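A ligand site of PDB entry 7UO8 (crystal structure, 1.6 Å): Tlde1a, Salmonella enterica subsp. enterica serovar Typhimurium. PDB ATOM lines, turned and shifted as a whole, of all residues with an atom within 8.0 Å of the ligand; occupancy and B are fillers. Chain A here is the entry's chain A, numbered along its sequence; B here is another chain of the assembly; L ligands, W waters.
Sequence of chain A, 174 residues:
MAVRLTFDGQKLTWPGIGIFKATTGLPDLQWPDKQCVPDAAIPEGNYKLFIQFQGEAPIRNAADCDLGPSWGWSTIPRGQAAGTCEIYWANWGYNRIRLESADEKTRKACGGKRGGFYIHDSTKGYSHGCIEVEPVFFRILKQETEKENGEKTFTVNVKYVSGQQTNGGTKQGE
The backbone carbonyl oxygen of Lys 113 lies close to a sulfur (S1) of the ligand. Residues that only touch the ligand: Pro 38, His 128, Gly 129, His 1 of chain B and His 3 of chain B. Ten residues have an atom within 4 Å of the ligand: Pro 38, Asp 39, Lys 113, Arg 114, Gly 115, His 128, Gly 129, His 1 of chain B, His 2 of chain B and His 3 of chain B. The nearest printed residue that does not touch the ligand is Phe 117 (4.2 Å).
NH2 of Arg 114 is in hydrogen-bond range of O of Ala 40 (2.9 Å). The backbone carbonyl oxygen of Val 37 lies within hydrogen-bond range of the guanidinium group of Arg 114. NH1 of Arg 114 lies within hydrogen-bond range of O of Ala 41, 2.8 Å away. NH1 of Arg 114 sits at hydrogen-bond distance from O of Gln 35 (2.7 Å). The backbone NH (N) of Gly 129 is in hydrogen-bond range of the backbone carbonyl oxygen (O) of Asp 39. O of Asp 39 is in hydrogen-bond range of N of Leu 26 (3.0 Å). A ring nitrogen (NE2) of His 3 of chain B lies within hydrogen-bond range of the backbone carbonyl oxygen of Gly 116 (2.6 Å). The side-chain sulfur of Cys 36 forms a disulfide with the side-chain sulfur of Cys 110 (2.0 Å).
The guanidinium group (NH2) of Arg 114 lies within salt-bridge range of an oxygen (O1) of the ligand, 2.8 Å away. An oxygen (O1) of the ligand lies within hydrogen-bond range of the backbone NH of Asp 39 (2.9 Å). The side-chain carboxylate (OD1) of Asp 39 is in salt-bridge range of a nitrogen (N1) of the ligand (3.0 Å). The backbone carbonyl oxygen of His 2 of chain B sits at hydrogen-bond distance from a nitrogen (N1) of the ligand. A sulfur (S1) of the ligand sits close to a ring nitrogen (ND1) of His 2 of chain B, at 3.6 Å. An oxygen (O2) of the ligand sits at hydrogen-bond distance from the backbone NH (N) of Gly 115, 3.2 Å away.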
ATOM      1  N   GLY A  25     -18.288 -19.942 -16.972  1.00  0.00           N
ATOM      2  CA  GLY A  25     -17.802 -19.193 -18.112  1.00  0.00           C
ATOM      3  C   GLY A  25     -17.722 -20.013 -19.388  1.00  0.00           C
ATOM      4  O   GLY A  25     -17.585 -21.250 -19.374  1.00  0.00           O
ATOM      5  N   LEU A  26     -17.796 -19.311 -20.523  1.00  0.00           N
ATOM      6  CA  LEU A  26     -17.605 -19.955 -21.811  1.00  0.00           C
ATOM      7  C   LEU A  26     -16.142 -20.352 -21.976  1.00  0.00           C
ATOM      8  O   LEU A  26     -15.277 -19.882 -21.245  1.00  0.00           O
ATOM      9  CB  LEU A  26     -18.049 -19.019 -22.941  1.00  0.00           C
ATOM     10  CG  LEU A  26     -19.573 -18.922 -23.105  1.00  0.00           C
ATOM     11  CD1 LEU A  26     -19.919 -17.941 -24.218  1.00  0.00           C
ATOM     12  CD2 LEU A  26     -20.181 -20.299 -23.381  1.00  0.00           C
ATOM     13  N   LEU A  29     -13.392 -17.816 -21.592  1.00  0.00           N
ATOM     14  CA  LEU A  29     -13.716 -16.766 -20.633  1.00  0.00           C
ATOM     15  C   LEU A  29     -13.725 -17.280 -19.191  1.00  0.00           C
ATOM     16  O   LEU A  29     -14.275 -16.624 -18.310  1.00  0.00           O
ATOM     17  CB  LEU A  29     -15.070 -16.144 -20.980  1.00  0.00           C
ATOM     18  CG  LEU A  29     -15.166 -15.498 -22.368  1.00  0.00           C
ATOM     19  CD1 LEU A  29     -16.603 -15.021 -22.609  1.00  0.00           C
ATOM     20  CD2 LEU A  29     -14.185 -14.356 -22.469  1.00  0.00           C
ATOM     21  N   GLN A  35     -14.316 -11.552 -15.449  1.00  0.00           N
ATOM     22  CA  GLN A  35     -15.620 -11.764 -14.833  1.00  0.00           C
ATOM     23  C   GLN A  35     -16.622 -10.659 -15.123  1.00  0.00           C
ATOM     24  O   GLN A  35     -17.784 -10.795 -14.707  1.00  0.00           O
ATOM     25  CB  GLN A  35     -15.453 -11.954 -13.326  1.00  0.00           C
ATOM     26  CG  GLN A  35     -15.056 -10.709 -12.578  1.00  0.00           C
ATOM     27  CD  GLN A  35     -14.818 -10.977 -11.099  1.00  0.00           C
ATOM     28  OE1 GLN A  35     -15.690 -10.719 -10.267  1.00  0.00           O
ATOM     29  NE2 GLN A  35     -13.638 -11.484 -10.761  1.00  0.00           N
ATOM     30  N   CYS A  36     -16.238  -9.588 -15.808  1.00  0.00           N
ATOM     31  CA  CYS A  36     -17.197  -8.576 -16.235  1.00  0.00           C
ATOM     32  C   CYS A  36     -17.471  -8.629 -17.726  1.00  0.00           C
ATOM     33  O   CYS A  36     -18.123  -7.720 -18.263  1.00  0.00           O
ATOM     34  CB  CYS A  36     -16.725  -7.196 -15.806  1.00  0.00           C
ATOM     35  SG  CYS A  36     -16.876  -6.934 -14.008  1.00  0.00           S
ATOM     36  N   VAL A  37     -16.991  -9.655 -18.413  1.00  0.00           N
ATOM     37  CA  VAL A  37     -17.306  -9.897 -19.820  1.00  0.00           C
ATOM     38  C   VAL A  37     -18.574 -10.731 -19.882  1.00  0.00           C
ATOM     39  O   VAL A  37     -18.714 -11.687 -19.100  1.00  0.00           O
ATOM     40  CB  VAL A  37     -16.137 -10.598 -20.539  1.00  0.00           C
ATOM     41  CG1 VAL A  37     -16.492 -10.913 -21.987  1.00  0.00           C
ATOM     42  CG2 VAL A  37     -14.871  -9.749 -20.469  1.00  0.00           C
ATOM     43  N   PRO A  38     -19.525 -10.419 -20.765  1.00  0.00           N
ATOM     44  CA  PRO A  38     -20.722 -11.261 -20.874  1.00  0.00           C
ATOM     45  C   PRO A  38     -20.349 -12.729 -21.085  1.00  0.00           C
ATOM     46  O   PRO A  38     -19.442 -13.062 -21.857  1.00  0.00           O
ATOM     47  CB  PRO A  38     -21.454 -10.693 -22.091  1.00  0.00           C
ATOM     48  CG  PRO A  38     -21.007  -9.259 -22.163  1.00  0.00           C
ATOM     49  CD  PRO A  38     -19.573  -9.265 -21.686  1.00  0.00           C
ATOM     50  N   ASP A  39     -21.073 -13.606 -20.388  1.00  0.00           N
ATOM     51  CA  ASP A  39     -20.945 -15.052 -20.477  1.00  0.00           C
ATOM     52  C   ASP A  39     -19.635 -15.580 -19.911  1.00  0.00           C
ATOM     53  O   ASP A  39     -19.346 -16.767 -20.072  1.00  0.00           O
ATOM     54  CB  ASP A  39     -21.098 -15.539 -21.927  1.00  0.00           C
ATOM     55  CG  ASP A  39     -22.503 -15.350 -22.456  1.00  0.00           C
ATOM     56  OD1 ASP A  39     -23.458 -15.498 -21.658  1.00  0.00           O
ATOM     57  OD2 ASP A  39     -22.644 -15.055 -23.668  1.00  0.00           O
ATOM     58  N   ALA A  40     -18.878 -14.763 -19.204  1.00  0.00           N
ATOM     59  CA  ALA A  40     -17.642 -15.199 -18.577  1.00  0.00           C
ATOM     60  C   ALA A  40     -17.914 -15.742 -17.174  1.00  0.00           C
ATOM     61  O   ALA A  40     -19.056 -15.820 -16.714  1.00  0.00           O
ATOM     62  CB  ALA A  40     -16.637 -14.042 -18.521  1.00  0.00           C
ATOM     63  N   ALA A  41     -16.837 -16.085 -16.466  1.00  0.00           N
ATOM     64  CA  ALA A  41     -16.936 -16.478 -15.066  1.00  0.00           C
ATOM     65  C   ALA A  41     -17.839 -15.505 -14.292  1.00  0.00           C
ATOM     66  O   ALA A  41     -17.766 -14.292 -14.457  1.00  0.00           O
ATOM     67  CB  ALA A  41     -15.544 -16.507 -14.433  1.00  0.00           C
ATOM     68  N   ILE A  42     -18.691 -16.079 -13.446  1.00  0.00           N
ATOM     69  CA  ILE A  42     -19.682 -15.280 -12.719  1.00  0.00           C
ATOM     70  C   ILE A  42     -18.978 -14.279 -11.801  1.00  0.00           C
ATOM     71  O   ILE A  42     -17.902 -14.588 -11.252  1.00  0.00           O
ATOM     72  CB  ILE A  42     -20.618 -16.213 -11.931  1.00  0.00           C
ATOM     73  CG1 ILE A  42     -21.742 -15.437 -11.244  1.00  0.00           C
ATOM     74  CG2 ILE A  42     -19.847 -17.024 -10.890  1.00  0.00           C
ATOM     75  CD1 ILE A  42     -22.832 -16.322 -10.689  1.00  0.00           C
ATOM     76  N   PRO A  43     -19.495 -13.057 -11.635  1.00  0.00           N
ATOM     77  CA  PRO A  43     -18.805 -12.080 -10.784  1.00  0.00           C
ATOM     78  C   PRO A  43     -18.772 -12.520  -9.324  1.00  0.00           C
ATOM     79  O   PRO A  43     -19.712 -13.143  -8.815  1.00  0.00           O
ATOM     80  CB  PRO A  43     -19.615 -10.791 -10.956  1.00  0.00           C
ATOM     81  CG  PRO A  43     -20.332 -10.958 -12.252  1.00  0.00           C
ATOM     82  CD  PRO A  43     -20.619 -12.440 -12.368  1.00  0.00           C
ATOM     83  N   CYS A 110     -19.416  -5.010 -12.011  1.00  0.00           N
ATOM     84  CA  CYS A 110     -19.491  -4.893 -13.466  1.00  0.00           C
ATOM     85  C   CYS A 110     -20.515  -3.864 -13.898  1.00  0.00           C
ATOM     86  O   CYS A 110     -21.208  -4.029 -14.905  1.00  0.00           O
ATOM     87  CB  CYS A 110     -19.804  -6.259 -14.098  1.00  0.00           C
ATOM     88  SG  CYS A 110     -18.737  -7.584 -13.540  1.00  0.00           S
ATOM     89  N   GLY A 112     -23.277  -3.336 -12.885  1.00  0.00           N
ATOM     90  CA  GLY A 112     -24.623  -3.862 -12.884  1.00  0.00           C
ATOM     91  C   GLY A 112     -25.101  -4.402 -14.206  1.00  0.00           C
ATOM     92  O   GLY A 112     -26.312  -4.606 -14.385  1.00  0.00           O
ATOM     93  N   LYS A 113     -24.196  -4.670 -15.146  1.00  0.00           N
ATOM     94  CA  LYS A 113     -24.579  -4.996 -16.506  1.00  0.00           C
ATOM     95  C   LYS A 113     -24.740  -6.486 -16.767  1.00  0.00           C
ATOM     96  O   LYS A 113     -25.192  -6.868 -17.856  1.00  0.00           O
ATOM     97  CB  LYS A 113     -23.538  -4.432 -17.484  1.00  0.00           C
ATOM     98  CG  LYS A 113     -23.389  -2.914 -17.433  1.00  0.00           C
ATOM     99  CD  LYS A 113     -24.679  -2.225 -17.843  1.00  0.00           C
ATOM    100  CE  LYS A 113     -24.513  -0.701 -17.872  1.00  0.00           C
ATOM    101  NZ  LYS A 113     -25.773  -0.022 -18.284  1.00  0.00           N
ATOM    102  N   ARG A 114     -24.387  -7.343 -15.807  1.00  0.00           N
ATOM    103  CA  ARG A 114     -24.519  -8.778 -15.970  1.00  0.00           C
ATOM    104  C   ARG A 114     -25.661  -9.307 -15.112  1.00  0.00           C
ATOM    105  O   ARG A 114     -26.116  -8.645 -14.178  1.00  0.00           O
ATOM    106  CB  ARG A 114     -23.211  -9.499 -15.596  1.00  0.00           C
ATOM    107  CG  ARG A 114     -22.077  -9.219 -16.570  1.00  0.00           C
ATOM    108  CD  ARG A 114     -20.946 -10.212 -16.378  1.00  0.00           C
ATOM    109  NE  ARG A 114     -21.360 -11.584 -16.642  1.00  0.00           N
ATOM    110  CZ  ARG A 114     -20.614 -12.652 -16.390  1.00  0.00           C
ATOM    111  NH1 ARG A 114     -19.400 -12.548 -15.885  1.00  0.00           N
ATOM    112  NH2 ARG A 114     -21.120 -13.856 -16.639  1.00  0.00           N
ATOM    113  N   GLY A 115     -26.106 -10.516 -15.437  1.00  0.00           N
ATOM    114  CA  GLY A 115     -27.201 -11.096 -14.694  1.00  0.00           C
ATOM    115  C   GLY A 115     -27.679 -12.397 -15.315  1.00  0.00           C
ATOM    116  O   GLY A 115     -27.024 -12.966 -16.181  1.00  0.00           O
ATOM    117  N   GLY A 116     -28.826 -12.852 -14.844  1.00  0.00           N
ATOM    118  CA  GLY A 116     -29.381 -14.100 -15.311  1.00  0.00           C
ATOM    119  C   GLY A 116     -28.634 -15.325 -14.844  1.00  0.00           C
ATOM    120  O   GLY A 116     -28.434 -16.264 -15.627  1.00  0.00           O
ATOM    121  N   PHE A 117     -28.163 -15.319 -13.595  1.00  0.00           N
ATOM    122  CA  PHE A 117     -27.262 -16.365 -13.129  1.00  0.00           C
ATOM    123  C   PHE A 117     -28.053 -17.549 -12.594  1.00  0.00           C
ATOM    124  O   PHE A 117     -29.100 -17.385 -11.947  1.00  0.00           O
ATOM    125  CB  PHE A 117     -26.340 -15.828 -12.039  1.00  0.00           C
ATOM    126  CG  PHE A 117     -25.581 -14.592 -12.420  1.00  0.00           C
ATOM    127  CD1 PHE A 117     -24.715 -14.625 -13.495  1.00  0.00           C
ATOM    128  CD2 PHE A 117     -25.723 -13.418 -11.706  1.00  0.00           C
ATOM    129  CE1 PHE A 117     -23.997 -13.485 -13.840  1.00  0.00           C
ATOM    130  CE2 PHE A 117     -25.015 -12.299 -12.052  1.00  0.00           C
ATOM    131  CZ  PHE A 117     -24.149 -12.331 -13.127  1.00  0.00           C
ATOM    132  N   SER A 127     -20.007 -22.858 -19.167  1.00  0.00           N
ATOM    133  CA  SER A 127     -21.305 -22.333 -18.798  1.00  0.00           C
ATOM    134  C   SER A 127     -21.457 -20.937 -19.380  1.00  0.00           C
ATOM    135  O   SER A 127     -20.518 -20.138 -19.310  1.00  0.00           O
ATOM    136  CB  SER A 127     -21.484 -22.300 -17.272  1.00  0.00           C
ATOM    137  OG  SER A 127     -22.726 -21.696 -16.942  1.00  0.00           O
ATOM    138  N   HIS A 128     -22.641 -20.655 -19.935  1.00  0.00           N
ATOM    139  CA  HIS A 128     -22.959 -19.344 -20.512  1.00  0.00           C
ATOM    140  C   HIS A 128     -23.216 -18.330 -19.405  1.00  0.00           C
ATOM    141  O   HIS A 128     -24.348 -17.887 -19.170  1.00  0.00           O
ATOM    142  CB  HIS A 128     -24.161 -19.429 -21.447  1.00  0.00           C
ATOM    143  CG  HIS A 128     -23.866 -20.088 -22.751  1.00  0.00           C
ATOM    144  ND1 HIS A 128     -23.705 -21.442 -22.892  1.00  0.00           N
ATOM    145  CD2 HIS A 128     -23.746 -19.565 -23.987  1.00  0.00           C
ATOM    146  CE1 HIS A 128     -23.458 -21.726 -24.166  1.00  0.00           C
ATOM    147  NE2 HIS A 128     -23.474 -20.605 -24.852  1.00  0.00           N
ATOM    148  N   GLY A 129     -22.142 -17.959 -18.711  1.00  0.00           N
ATOM    149  CA  GLY A 129     -22.245 -16.952 -17.647  1.00  0.00           C
ATOM    150  C   GLY A 129     -22.949 -17.417 -16.386  1.00  0.00           C
ATOM    151  O   GLY A 129     -23.534 -16.610 -15.678  1.00  0.00           O
ATOM    152  N   CME A 130     -22.879 -18.701 -16.104  1.00  0.00           N
ATOM    153  CA  CME A 130     -23.495 -19.323 -14.940  1.00  0.00           C
ATOM    154  CB  CME A 130     -24.823 -19.967 -15.311  1.00  0.00           C
ATOM    155  SG  CME A 130     -26.010 -18.841 -16.054  1.00  0.00           S
ATOM    156  SD  CME A 130     -27.504 -20.061 -16.788  1.00  0.00           S
ATOM    157  CE  CME A 130     -27.245 -20.310 -18.507  1.00  0.00           C
ATOM    158  CZ  CME A 130     -26.823 -21.751 -18.833  1.00  0.00           C
ATOM    159  OH  CME A 130     -26.614 -21.845 -20.242  1.00  0.00           O
ATOM    160  C   CME A 130     -22.518 -20.299 -14.335  1.00  0.00           C
ATOM    161  O   CME A 130     -21.328 -20.288 -14.628  1.00  0.00           O
ATOM    162  N   HIS B   1     -32.390  -9.319 -22.735  1.00  0.00           N
ATOM    163  CA  HIS B   1     -32.412 -10.580 -21.981  1.00  0.00           C
ATOM    164  C   HIS B   1     -31.009 -11.048 -21.689  1.00  0.00           C
ATOM    165  O   HIS B   1     -30.050 -10.622 -22.331  1.00  0.00           O
ATOM    166  CB  HIS B   1     -33.183 -11.646 -22.754  1.00  0.00           C
ATOM    167  CG  HIS B   1     -34.603 -11.264 -23.049  1.00  0.00           C
ATOM    168  ND1 HIS B   1     -35.310 -11.787 -24.116  1.00  0.00           N
ATOM    169  CD2 HIS B   1     -35.451 -10.424 -22.419  1.00  0.00           C
ATOM    170  CE1 HIS B   1     -36.530 -11.274 -24.121  1.00  0.00           C
ATOM    171  NE2 HIS B   1     -36.638 -10.442 -23.102  1.00  0.00           N
ATOM    172  N   HIS B   2     -30.805 -11.603 -20.488  1.00  0.00           N
ATOM    173  CA  HIS B   2     -29.492 -12.126 -20.122  1.00  0.00           C
ATOM    174  C   HIS B   2     -29.110 -13.341 -20.952  1.00  0.00           C
ATOM    175  O   HIS B   2     -27.922 -13.637 -21.069  1.00  0.00           O
ATOM    176  CB  HIS B   2     -29.466 -12.475 -18.638  1.00  0.00           C
ATOM    177  CG  HIS B   2     -29.856 -11.340 -17.736  1.00  0.00           C
ATOM    178  ND1 HIS B   2     -29.073 -10.221 -17.576  1.00  0.00           N
ATOM    179  CD2 HIS B   2     -30.935 -11.164 -16.948  1.00  0.00           C
ATOM    180  CE1 HIS B   2     -29.652  -9.400 -16.724  1.00  0.00           C
ATOM    181  NE2 HIS B   2     -30.789  -9.945 -16.328  1.00  0.00           N
ATOM    182  N   HIS B   3     -30.086 -14.045 -21.516  1.00  0.00           N
ATOM    183  CA  HIS B   3     -29.843 -15.245 -22.299  1.00  0.00           C
ATOM    184  C   HIS B   3     -30.727 -15.214 -23.537  1.00  0.00           C
ATOM    185  O   HIS B   3     -31.824 -14.652 -23.527  1.00  0.00           O
ATOM    186  CB  HIS B   3     -30.107 -16.515 -21.496  1.00  0.00           C
ATOM    187  CG  HIS B   3     -29.301 -16.627 -20.242  1.00  0.00           C
ATOM    188  ND1 HIS B   3     -27.963 -16.953 -20.244  1.00  0.00           N
ATOM    189  CD2 HIS B   3     -29.646 -16.427 -18.940  1.00  0.00           C
ATOM    190  CE1 HIS B   3     -27.516 -16.951 -18.993  1.00  0.00           C
ATOM    191  NE2 HIS B   3     -28.514 -16.636 -18.192  1.00  0.00           N
ATOM    192  N   HIS B   4     -30.238 -15.841 -24.603  1.00  0.00           N
ATOM    193  CA  HIS B   4     -31.012 -16.009 -25.835  1.00  0.00           C
ATOM    194  C   HIS B   4     -31.499 -17.429 -26.023  1.00  0.00           C
ATOM    195  O   HIS B   4     -32.302 -17.680 -26.939  1.00  0.00           O
ATOM    196  CB  HIS B   4     -30.170 -15.588 -27.052  1.00  0.00           C
ATOM    197  CG  HIS B   4     -29.819 -14.135 -27.067  1.00  0.00           C
ATOM    198  ND1 HIS B   4     -28.797 -13.613 -27.838  1.00  0.00           N
ATOM    199  CD2 HIS B   4     -30.380 -13.092 -26.423  1.00  0.00           C
ATOM    200  CE1 HIS B   4     -28.726 -12.314 -27.641  1.00  0.00           C
ATOM    201  NE2 HIS B   4     -29.656 -11.966 -26.768  1.00  0.00           N
HETATM  202  N1  LIG L   1     -25.456 -14.261 -19.739  1.00  0.00           N
HETATM  203  C1  LIG L   1     -25.309 -12.854 -19.391  1.00  0.00           C
HETATM  204  C2  LIG L   1     -24.136 -12.695 -18.437  1.00  0.00           C
HETATM  205  O1  LIG L   1     -23.195 -13.493 -18.476  1.00  0.00           O
HETATM  206  C3  LIG L   1     -25.069 -12.010 -20.637  1.00  0.00           C
HETATM  207  C4  LIG L   1     -24.872 -10.519 -20.348  1.00  0.00           C
HETATM  208  S1  LIG L   1     -26.359  -9.648 -19.797  1.00  0.00           S
HETATM  209  C5  LIG L   1     -27.203  -9.390 -21.373  1.00  0.00           C
HETATM  210  O2  LIG L   1     -24.110 -11.752 -17.622  1.00  0.00           O
HETATM  211  O   HOH W   1     -25.623 -15.264 -17.166  1.00  0.00           O
